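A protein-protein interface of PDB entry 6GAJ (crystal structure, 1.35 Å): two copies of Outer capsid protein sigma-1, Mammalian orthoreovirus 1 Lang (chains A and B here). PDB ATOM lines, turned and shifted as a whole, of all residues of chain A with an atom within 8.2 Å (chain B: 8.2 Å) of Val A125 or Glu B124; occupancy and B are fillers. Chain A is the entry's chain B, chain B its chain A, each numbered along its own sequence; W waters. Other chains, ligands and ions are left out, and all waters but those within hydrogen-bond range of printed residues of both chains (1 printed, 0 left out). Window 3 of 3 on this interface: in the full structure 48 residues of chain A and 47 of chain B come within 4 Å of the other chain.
Thr A118 touches Leu B117.
CZ of Arg B120 touches CG1 of Val A121 (3.6 Å).
CG2 of Val B121 touches CG2 of Val A121 (3.8 Å).
CG1 of Val A125 touches OE1 of Glu B124, 3.2 Å away.
NH2 of Arg B127 touches CG1 of Val A125 (3.3 Å).
Leu B128 touches Leu A128.
OD1 of Asp A129 touches CD2 of Leu B128 (3.4 Å).
Asp A129 touches Leu B131.
Ile A132 touches Leu B128.
CG2 of Ile A132 touches CB of Leu B131 (3.8 Å).
Of the 15 printed residues of chain B, 7 touch a printed residue of chain A.
Printed residues of chain B that touch a printed residue of chain A: Leu B117, Arg B120, Val B121, Glu B124, Arg B127, Leu B128 and Leu B131.
Of the 15 printed residues of chain A, 7 touch a printed residue of chain B.
Printed residues of chain A that touch a printed residue of chain B: Thr A118, Val A121, Thr A122, Val A125, Leu A128, Asp A129 and Ile A132.
Hydrophobic or aromatic side chains of chain A that line the printed part of chain B: Val A121, Val A125, Leu A128 and Ile A132.
Of the printed residues of chain A, Glu B124 touches Val A125 (3.2 Å).
Printed residues of chain B within 4 Å of Asp A129: Arg B127 (2.7 Å), Leu B128 (3.4 Å) and Leu B131 (3.6 Å).
Of the printed residues of chain B, Thr A122 touches Arg B120 (2.7 Å).
Of the printed residues of chain A, Leu B131 touches Asp A129 and Ile A132.
OE2 of Glu B124 is in salt-bridge range of NE of Arg B127.
The side-chain hydroxyl (OG1) of Thr A122 is in hydrogen-bond range of the backbone carbonyl oxygen (O) of Thr A118 (3.4 Å).
The side-chain hydroxyl (OG1) of Thr A126 lies within hydrogen-bond range of the backbone carbonyl oxygen (O) of Thr A122 (2.8 Å).
Water W1 lies within hydrogen-bond range of OG1 of Thr A122 (3.0 Å) and NH2 of Arg B120 (3.2 Å).
Thr A122 touches Arg B120, but with the chains exchanged Arg A120 does not touch Thr B122 (12.0 Å).
Val A125 touches Arg B127, but with the chains exchanged Arg A127 does not touch Val B125 (10.9 Å).
Leu B128 touches its own counterpart, Leu A128.
Asp A129 touches Leu B128, but with the chains exchanged Leu A128 does not touch Asp B129 (8.0 Å).
14 positions are printed for both chains.
Of the 13 pairs that touch across the chains among the printed residues, 2 have their exchanged pair printed and touching as well.
NH1 of Arg B120 lies within hydrogen-bond range of O of Thr A118 (3.3 Å).
The side-chain hydroxyl of Thr A122 is in hydrogen-bond range of the guanidinium group of Arg B120 (2.7 Å).
The guanidinium group (NH2) of Arg B127 is in salt-bridge range of the side-chain carboxylate (OD2) of Asp A129 (2.7 Å).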
ATOM      1  N   THR A 118     -17.733   0.270 -12.638  1.00  0.00           N
ATOM      2  CA  THR A 118     -18.340   0.533 -13.940  1.00  0.00           C
ATOM      3  C   THR A 118     -19.026   1.904 -13.903  1.00  0.00           C
ATOM      4  O   THR A 118     -18.837   2.737 -14.784  1.00  0.00           O
ATOM      5  CB  THR A 118     -19.353  -0.570 -14.273  1.00  0.00           C
ATOM      6  OG1 THR A 118     -18.658  -1.820 -14.369  1.00  0.00           O
ATOM      7  CG2 THR A 118     -20.091  -0.299 -15.572  1.00  0.00           C
ATOM      8  N   THR A 119     -19.794   2.142 -12.828  1.00  0.00           N
ATOM      9  CA  THR A 119     -20.493   3.437 -12.647  1.00  0.00           C
ATOM     10  C   THR A 119     -19.439   4.562 -12.521  1.00  0.00           C
ATOM     11  O   THR A 119     -19.603   5.656 -13.053  1.00  0.00           O
ATOM     12  CB  THR A 119     -21.341   3.332 -11.380  1.00  0.00           C
ATOM     13  OG1 THR A 119     -22.342   2.325 -11.549  1.00  0.00           O
ATOM     14  CG2 THR A 119     -21.953   4.705 -10.933  1.00  0.00           C
ATOM     15  N   ARG A 120     -18.350   4.322 -11.743  1.00  0.00           N
ATOM     16  CA  ARG A 120     -17.308   5.329 -11.527  1.00  0.00           C
ATOM     17  C   ARG A 120     -16.651   5.741 -12.863  1.00  0.00           C
ATOM     18  O   ARG A 120     -16.418   6.909 -13.124  1.00  0.00           O
ATOM     19  CB  ARG A 120     -16.280   4.824 -10.525  1.00  0.00           C
ATOM     20  CG  ARG A 120     -15.139   5.768 -10.327  1.00  0.00           C
ATOM     21  CD  ARG A 120     -14.220   5.261  -9.234  1.00  0.00           C
ATOM     22  NE  ARG A 120     -13.116   6.217  -9.140  1.00  0.00           N
ATOM     23  CZ  ARG A 120     -11.828   5.891  -9.073  1.00  0.00           C
ATOM     24  NH1 ARG A 120     -11.452   4.601  -9.059  1.00  0.00           N
ATOM     25  NH2 ARG A 120     -10.905   6.845  -9.057  1.00  0.00           N
ATOM     26  N   VAL A 121     -16.363   4.753 -13.729  1.00  0.00           N
ATOM     27  CA  VAL A 121     -15.744   5.085 -15.027  1.00  0.00           C
ATOM     28  C   VAL A 121     -16.722   5.986 -15.781  1.00  0.00           C
ATOM     29  O   VAL A 121     -16.316   7.011 -16.330  1.00  0.00           O
ATOM     30  CB  VAL A 121     -15.387   3.832 -15.806  1.00  0.00           C
ATOM     31  CG1 VAL A 121     -14.987   4.155 -17.246  1.00  0.00           C
ATOM     32  CG2 VAL A 121     -14.286   3.033 -15.079  1.00  0.00           C
ATOM     33  N   THR A 122     -18.053   5.640 -15.766  1.00  0.00           N
ATOM     34  CA  THR A 122     -18.990   6.543 -16.456  1.00  0.00           C
ATOM     35  C   THR A 122     -19.000   7.909 -15.853  1.00  0.00           C
ATOM     36  O   THR A 122     -18.929   8.910 -16.605  1.00  0.00           O
ATOM     37  CB  THR A 122     -20.383   5.911 -16.428  1.00  0.00           C
ATOM     38  OG1 THR A 122     -20.306   4.674 -17.135  1.00  0.00           O
ATOM     39  CG2 THR A 122     -21.427   6.865 -17.100  1.00  0.00           C
ATOM     40  N   THR A 123     -19.059   8.031 -14.523  1.00  0.00           N
ATOM     41  CA  THR A 123     -19.078   9.327 -13.826  1.00  0.00           C
ATOM     42  C   THR A 123     -17.881  10.147 -14.245  1.00  0.00           C
ATOM     43  O   THR A 123     -18.018  11.331 -14.614  1.00  0.00           O
ATOM     44  CB  THR A 123     -19.062   9.085 -12.295  1.00  0.00           C
ATOM     45  OG1 THR A 123     -20.264   8.432 -11.960  1.00  0.00           O
ATOM     46  CG2 THR A 123     -18.966  10.433 -11.475  1.00  0.00           C
ATOM     47  N   GLU A 124     -16.673   9.562 -14.160  1.00  0.00           N
ATOM     48  CA  GLU A 124     -15.486  10.367 -14.411  1.00  0.00           C
ATOM     49  C   GLU A 124     -15.303  10.711 -15.860  1.00  0.00           C
ATOM     50  O   GLU A 124     -14.903  11.853 -16.166  1.00  0.00           O
ATOM     51  CB  GLU A 124     -14.219   9.638 -13.901  1.00  0.00           C
ATOM     52  CG  GLU A 124     -14.259   9.472 -12.366  1.00  0.00           C
ATOM     53  CD  GLU A 124     -14.274  10.792 -11.592  1.00  0.00           C
ATOM     54  OE1 GLU A 124     -13.864  11.853 -12.118  1.00  0.00           O
ATOM     55  OE2 GLU A 124     -14.873  10.778 -10.500  1.00  0.00           O
ATOM     56  N   VAL A 125     -15.630   9.785 -16.777  1.00  0.00           N
ATOM     57  CA  VAL A 125     -15.482  10.077 -18.219  1.00  0.00           C
ATOM     58  C   VAL A 125     -16.519  11.168 -18.604  1.00  0.00           C
ATOM     59  O   VAL A 125     -16.200  12.127 -19.342  1.00  0.00           O
ATOM     60  CB  VAL A 125     -15.637   8.832 -19.065  1.00  0.00           C
ATOM     61  CG1 VAL A 125     -15.798   9.162 -20.557  1.00  0.00           C
ATOM     62  CG2 VAL A 125     -14.467   7.881 -18.823  1.00  0.00           C
ATOM     63  N   THR A 126     -17.756  11.080 -18.072  1.00  0.00           N
ATOM     64  CA  THR A 126     -18.753  12.099 -18.379  1.00  0.00           C
ATOM     65  C   THR A 126     -18.274  13.475 -17.901  1.00  0.00           C
ATOM     66  O   THR A 126     -18.380  14.478 -18.655  1.00  0.00           O
ATOM     67  CB  THR A 126     -20.105  11.727 -17.718  1.00  0.00           C
ATOM     68  OG1 THR A 126     -20.571  10.504 -18.242  1.00  0.00           O
ATOM     69  CG2 THR A 126     -21.178  12.813 -17.970  1.00  0.00           C
ATOM     70  N   ARG A 127     -17.705  13.533 -16.723  1.00  0.00           N
ATOM     71  CA  ARG A 127     -17.179  14.758 -16.120  1.00  0.00           C
ATOM     72  C   ARG A 127     -16.058  15.345 -16.970  1.00  0.00           C
ATOM     73  O   ARG A 127     -16.122  16.545 -17.371  1.00  0.00           O
ATOM     74  CB  ARG A 127     -16.709  14.499 -14.707  1.00  0.00           C
ATOM     75  CG  ARG A 127     -16.311  15.795 -13.992  1.00  0.00           C
ATOM     76  CD  ARG A 127     -15.772  15.520 -12.583  1.00  0.00           C
ATOM     77  NE  ARG A 127     -14.608  14.627 -12.590  1.00  0.00           N
ATOM     78  CZ  ARG A 127     -13.379  14.992 -12.927  1.00  0.00           C
ATOM     79  NH1 ARG A 127     -13.115  16.261 -13.253  1.00  0.00           N
ATOM     80  NH2 ARG A 127     -12.396  14.102 -12.935  1.00  0.00           N
ATOM     81  N   LEU A 128     -15.036  14.531 -17.308  1.00  0.00           N
ATOM     82  CA  LEU A 128     -13.924  15.002 -18.125  1.00  0.00           C
ATOM     83  C   LEU A 128     -14.405  15.483 -19.505  1.00  0.00           C
ATOM     84  O   LEU A 128     -13.964  16.563 -19.999  1.00  0.00           O
ATOM     85  CB  LEU A 128     -12.900  13.895 -18.265  1.00  0.00           C
ATOM     86  CG  LEU A 128     -12.140  13.588 -16.976  1.00  0.00           C
ATOM     87  CD1 LEU A 128     -11.385  12.228 -17.043  1.00  0.00           C
ATOM     88  CD2 LEU A 128     -11.130  14.707 -16.567  1.00  0.00           C
ATOM     89  N   ASP A 129     -15.288  14.734 -20.155  1.00  0.00           N
ATOM     90  CA  ASP A 129     -15.807  15.122 -21.478  1.00  0.00           C
ATOM     91  C   ASP A 129     -16.501  16.491 -21.377  1.00  0.00           C
ATOM     92  O   ASP A 129     -16.341  17.308 -22.284  1.00  0.00           O
ATOM     93  CB  ASP A 129     -16.861  14.127 -21.967  1.00  0.00           C
ATOM     94  CG  ASP A 129     -16.360  13.102 -22.946  1.00  0.00           C
ATOM     95  OD1 ASP A 129     -15.520  13.456 -23.803  1.00  0.00           O
ATOM     96  OD2 ASP A 129     -16.791  11.928 -22.851  1.00  0.00           O
ATOM     97  N   GLY A 130     -17.181  16.763 -20.259  1.00  0.00           N
ATOM     98  CA  GLY A 130     -17.896  18.013 -20.110  1.00  0.00           C
ATOM     99  C   GLY A 130     -16.955  19.190 -19.974  1.00  0.00           C
ATOM    100  O   GLY A 130     -17.347  20.330 -20.304  1.00  0.00           O
ATOM    101  N   LEU A 131     -15.738  18.958 -19.442  1.00  0.00           N
ATOM    102  CA  LEU A 131     -14.709  19.990 -19.251  1.00  0.00           C
ATOM    103  C   LEU A 131     -14.012  20.299 -20.551  1.00  0.00           C
ATOM    104  O   LEU A 131     -13.395  21.361 -20.626  1.00  0.00           O
ATOM    105  CB  LEU A 131     -13.681  19.590 -18.157  1.00  0.00           C
ATOM    106  CG  LEU A 131     -14.216  19.414 -16.725  1.00  0.00           C
ATOM    107  CD1 LEU A 131     -13.142  18.810 -15.766  1.00  0.00           C
ATOM    108  CD2 LEU A 131     -14.748  20.759 -16.129  1.00  0.00           C
ATOM    109  N   ILE A 132     -14.070  19.405 -21.566  1.00  0.00           N
ATOM    110  CA  ILE A 132     -13.354  19.608 -22.830  1.00  0.00           C
ATOM    111  C   ILE A 132     -14.227  20.351 -23.836  1.00  0.00           C
ATOM    112  O   ILE A 132     -15.281  19.854 -24.255  1.00  0.00           O
ATOM    113  CB  ILE A 132     -12.790  18.251 -23.378  1.00  0.00           C
ATOM    114  CG1 ILE A 132     -11.843  17.575 -22.362  1.00  0.00           C
ATOM    115  CG2 ILE A 132     -12.101  18.483 -24.730  1.00  0.00           C
ATOM    116  CD1 ILE A 132     -11.663  15.998 -22.643  1.00  0.00           C
ATOM    117  N   LEU B 117     -14.279  -4.042 -19.078  1.00  0.00           N
ATOM    118  CA  LEU B 117     -14.130  -2.729 -18.433  1.00  0.00           C
ATOM    119  C   LEU B 117     -12.673  -2.228 -18.530  1.00  0.00           C
ATOM    120  O   LEU B 117     -12.433  -1.040 -18.752  1.00  0.00           O
ATOM    121  CB  LEU B 117     -14.606  -2.843 -16.985  1.00  0.00           C
ATOM    122  CG  LEU B 117     -14.619  -1.503 -16.233  1.00  0.00           C
ATOM    123  CD1 LEU B 117     -15.577  -0.524 -16.877  1.00  0.00           C
ATOM    124  CD2 LEU B 117     -14.974  -1.688 -14.735  1.00  0.00           C
ATOM    125  N   THR B 118     -11.690  -3.129 -18.449  1.00  0.00           N
ATOM    126  CA  THR B 118     -10.280  -2.773 -18.661  1.00  0.00           C
ATOM    127  C   THR B 118     -10.106  -2.179 -20.081  1.00  0.00           C
ATOM    128  O   THR B 118      -9.489  -1.118 -20.233  1.00  0.00           O
ATOM    129  CB  THR B 118      -9.453  -4.025 -18.498  1.00  0.00           C
ATOM    130  OG1 THR B 118      -9.620  -4.522 -17.148  1.00  0.00           O
ATOM    131  CG2 THR B 118      -7.992  -3.770 -18.789  1.00  0.00           C
ATOM    132  N   THR B 119     -10.700  -2.819 -21.096  1.00  0.00           N
ATOM    133  CA  THR B 119     -10.599  -2.333 -22.486  1.00  0.00           C
ATOM    134  C   THR B 119     -11.318  -0.973 -22.554  1.00  0.00           C
ATOM    135  O   THR B 119     -10.835  -0.059 -23.241  1.00  0.00           O
ATOM    136  CB  THR B 119     -11.278  -3.403 -23.384  1.00  0.00           C
ATOM    137  OG1 THR B 119     -10.520  -4.609 -23.352  1.00  0.00           O
ATOM    138  CG2 THR B 119     -11.440  -2.942 -24.890  1.00  0.00           C
ATOM    139  N   ARG B 120     -12.490  -0.821 -21.924  1.00  0.00           N
ATOM    140  CA  ARG B 120     -13.251   0.428 -21.970  1.00  0.00           C
ATOM    141  C   ARG B 120     -12.398   1.574 -21.355  1.00  0.00           C
ATOM    142  O   ARG B 120     -12.357   2.657 -21.925  1.00  0.00           O
ATOM    143  CB  ARG B 120     -14.559   0.244 -21.228  1.00  0.00           C
ATOM    144  CG  ARG B 120     -15.336   1.528 -21.059  1.00  0.00           C
ATOM    145  CD  ARG B 120     -16.612   1.294 -20.284  1.00  0.00           C
ATOM    146  NE  ARG B 120     -17.226   2.600 -20.069  1.00  0.00           N
ATOM    147  CZ  ARG B 120     -17.894   2.998 -18.997  1.00  0.00           C
ATOM    148  NH1 ARG B 120     -18.094   2.157 -17.960  1.00  0.00           N
ATOM    149  NH2 ARG B 120     -18.354   4.246 -18.933  1.00  0.00           N
ATOM    150  N   VAL B 121     -11.731   1.343 -20.219  1.00  0.00           N
ATOM    151  CA  VAL B 121     -10.889   2.395 -19.637  1.00  0.00           C
ATOM    152  C   VAL B 121      -9.793   2.787 -20.658  1.00  0.00           C
ATOM    153  O   VAL B 121      -9.563   3.962 -20.906  1.00  0.00           O
ATOM    154  CB  VAL B 121     -10.286   1.942 -18.299  1.00  0.00           C
ATOM    155  CG1 VAL B 121      -9.174   2.905 -17.789  1.00  0.00           C
ATOM    156  CG2 VAL B 121     -11.429   1.763 -17.254  1.00  0.00           C
ATOM    157  N   THR B 122      -9.153   1.805 -21.315  1.00  0.00           N
ATOM    158  CA  THR B 122      -8.151   2.153 -22.338  1.00  0.00           C
ATOM    159  C   THR B 122      -8.780   2.952 -23.478  1.00  0.00           C
ATOM    160  O   THR B 122      -8.189   4.006 -23.858  1.00  0.00           O
ATOM    161  CB  THR B 122      -7.532   0.850 -22.859  1.00  0.00           C
ATOM    162  OG1 THR B 122      -6.901   0.210 -21.813  1.00  0.00           O
ATOM    163  CG2 THR B 122      -6.512   1.134 -24.042  1.00  0.00           C
ATOM    164  N   THR B 123      -9.916   2.519 -24.033  1.00  0.00           N
ATOM    165  CA  THR B 123     -10.617   3.186 -25.153  1.00  0.00           C
ATOM    166  C   THR B 123     -10.940   4.636 -24.742  1.00  0.00           C
ATOM    167  O   THR B 123     -10.660   5.602 -25.496  1.00  0.00           O
ATOM    168  CB  THR B 123     -11.945   2.430 -25.456  1.00  0.00           C
ATOM    169  OG1 THR B 123     -11.635   1.140 -25.929  1.00  0.00           O
ATOM    170  CG2 THR B 123     -12.838   3.175 -26.509  1.00  0.00           C
ATOM    171  N   GLU B 124     -11.509   4.812 -23.551  1.00  0.00           N
ATOM    172  CA  GLU B 124     -11.953   6.136 -23.143  1.00  0.00           C
ATOM    173  C   GLU B 124     -10.799   7.055 -22.781  1.00  0.00           C
ATOM    174  O   GLU B 124     -10.869   8.254 -23.157  1.00  0.00           O
ATOM    175  CB  GLU B 124     -12.953   6.046 -21.999  1.00  0.00           C
ATOM    176  CG  GLU B 124     -14.249   5.351 -22.406  1.00  0.00           C
ATOM    177  CD  GLU B 124     -15.045   6.156 -23.419  1.00  0.00           C
ATOM    178  OE1 GLU B 124     -15.857   6.976 -22.959  1.00  0.00           O
ATOM    179  OE2 GLU B 124     -14.725   6.159 -24.628  1.00  0.00           O
ATOM    180  N   VAL B 125      -9.725   6.571 -22.150  1.00  0.00           N
ATOM    181  CA  VAL B 125      -8.574   7.420 -21.843  1.00  0.00           C
ATOM    182  C   VAL B 125      -7.909   7.822 -23.196  1.00  0.00           C
ATOM    183  O   VAL B 125      -7.565   8.985 -23.369  1.00  0.00           O
ATOM    184  CB  VAL B 125      -7.614   6.695 -20.924  1.00  0.00           C
ATOM    185  CG1 VAL B 125      -6.269   7.411 -20.868  1.00  0.00           C
ATOM    186  CG2 VAL B 125      -8.222   6.510 -19.502  1.00  0.00           C
ATOM    187  N   THR B 126      -7.787   6.896 -24.160  1.00  0.00           N
ATOM    188  CA  THR B 126      -7.206   7.299 -25.466  1.00  0.00           C
ATOM    189  C   THR B 126      -8.082   8.425 -26.103  1.00  0.00           C
ATOM    190  O   THR B 126      -7.536   9.456 -26.599  1.00  0.00           O
ATOM    191  CB  THR B 126      -7.226   6.052 -26.420  1.00  0.00           C
ATOM    192  OG1 THR B 126      -6.289   5.150 -25.929  1.00  0.00           O
ATOM    193  CG2 THR B 126      -6.816   6.433 -27.886  1.00  0.00           C
ATOM    194  N   ARG B 127      -9.375   8.287 -26.071  1.00  0.00           N
ATOM    195  CA  ARG B 127     -10.315   9.228 -26.636  1.00  0.00           C
ATOM    196  C   ARG B 127     -10.168  10.597 -25.953  1.00  0.00           C
ATOM    197  O   ARG B 127     -10.011  11.643 -26.631  1.00  0.00           O
ATOM    198  CB  ARG B 127     -11.748   8.741 -26.519  1.00  0.00           C
ATOM    199  CG  ARG B 127     -12.737   9.624 -27.246  1.00  0.00           C
ATOM    200  CD  ARG B 127     -14.166   9.133 -27.124  1.00  0.00           C
ATOM    201  NE  ARG B 127     -14.586   9.064 -25.725  1.00  0.00           N
ATOM    202  CZ  ARG B 127     -14.912  10.114 -24.978  1.00  0.00           C
ATOM    203  NH1 ARG B 127     -14.911  11.340 -25.500  1.00  0.00           N
ATOM    204  NH2 ARG B 127     -15.228   9.952 -23.705  1.00  0.00           N
ATOM    205  N   LEU B 128     -10.198  10.639 -24.605  1.00  0.00           N
ATOM    206  CA  LEU B 128     -10.071  11.916 -23.879  1.00  0.00           C
ATOM    207  C   LEU B 128      -8.710  12.551 -24.118  1.00  0.00           C
ATOM    208  O   LEU B 128      -8.634  13.754 -24.338  1.00  0.00           O
ATOM    209  CB  LEU B 128     -10.277  11.637 -22.382  1.00  0.00           C
ATOM    210  CG  LEU B 128     -11.696  11.257 -22.019  1.00  0.00           C
ATOM    211  CD1 LEU B 128     -11.744  10.696 -20.587  1.00  0.00           C
ATOM    212  CD2 LEU B 128     -12.664  12.461 -22.151  1.00  0.00           C
ATOM    213  N   ASP B 129      -7.630  11.775 -24.132  1.00  0.00           N
ATOM    214  CA  ASP B 129      -6.305  12.335 -24.398  1.00  0.00           C
ATOM    215  C   ASP B 129      -6.315  12.994 -25.785  1.00  0.00           C
ATOM    216  O   ASP B 129      -5.724  14.060 -25.945  1.00  0.00           O
ATOM    217  CB  ASP B 129      -5.237  11.211 -24.426  1.00  0.00           C
ATOM    218  CG  ASP B 129      -4.435  11.082 -23.147  1.00  0.00           C
ATOM    219  OD1 ASP B 129      -4.088  12.107 -22.544  1.00  0.00           O
ATOM    220  OD2 ASP B 129      -4.170   9.924 -22.715  1.00  0.00           O
ATOM    221  N   GLY B 130      -6.980  12.368 -26.767  1.00  0.00           N
ATOM    222  CA  GLY B 130      -7.061  12.887 -28.146  1.00  0.00           C
ATOM    223  C   GLY B 130      -7.735  14.231 -28.207  1.00  0.00           C
ATOM    224  O   GLY B 130      -7.406  15.056 -29.067  1.00  0.00           O
ATOM    225  N   LEU B 131      -8.731  14.445 -27.368  1.00  0.00           N
ATOM    226  CA  LEU B 131      -9.493  15.694 -27.324  1.00  0.00           C
ATOM    227  C   LEU B 131      -8.735  16.797 -26.619  1.00  0.00           C
ATOM    228  O   LEU B 131      -8.990  17.968 -26.949  1.00  0.00           O
ATOM    229  CB  LEU B 131     -10.875  15.473 -26.647  1.00  0.00           C
ATOM    230  CG  LEU B 131     -11.855  14.492 -27.314  1.00  0.00           C
ATOM    231  CD1 LEU B 131     -13.090  14.230 -26.401  1.00  0.00           C
ATOM    232  CD2 LEU B 131     -12.353  15.050 -28.636  1.00  0.00           C
HETATM  233  O   HOH W   1     -21.239   5.125 -19.958  1.00  0.00           O
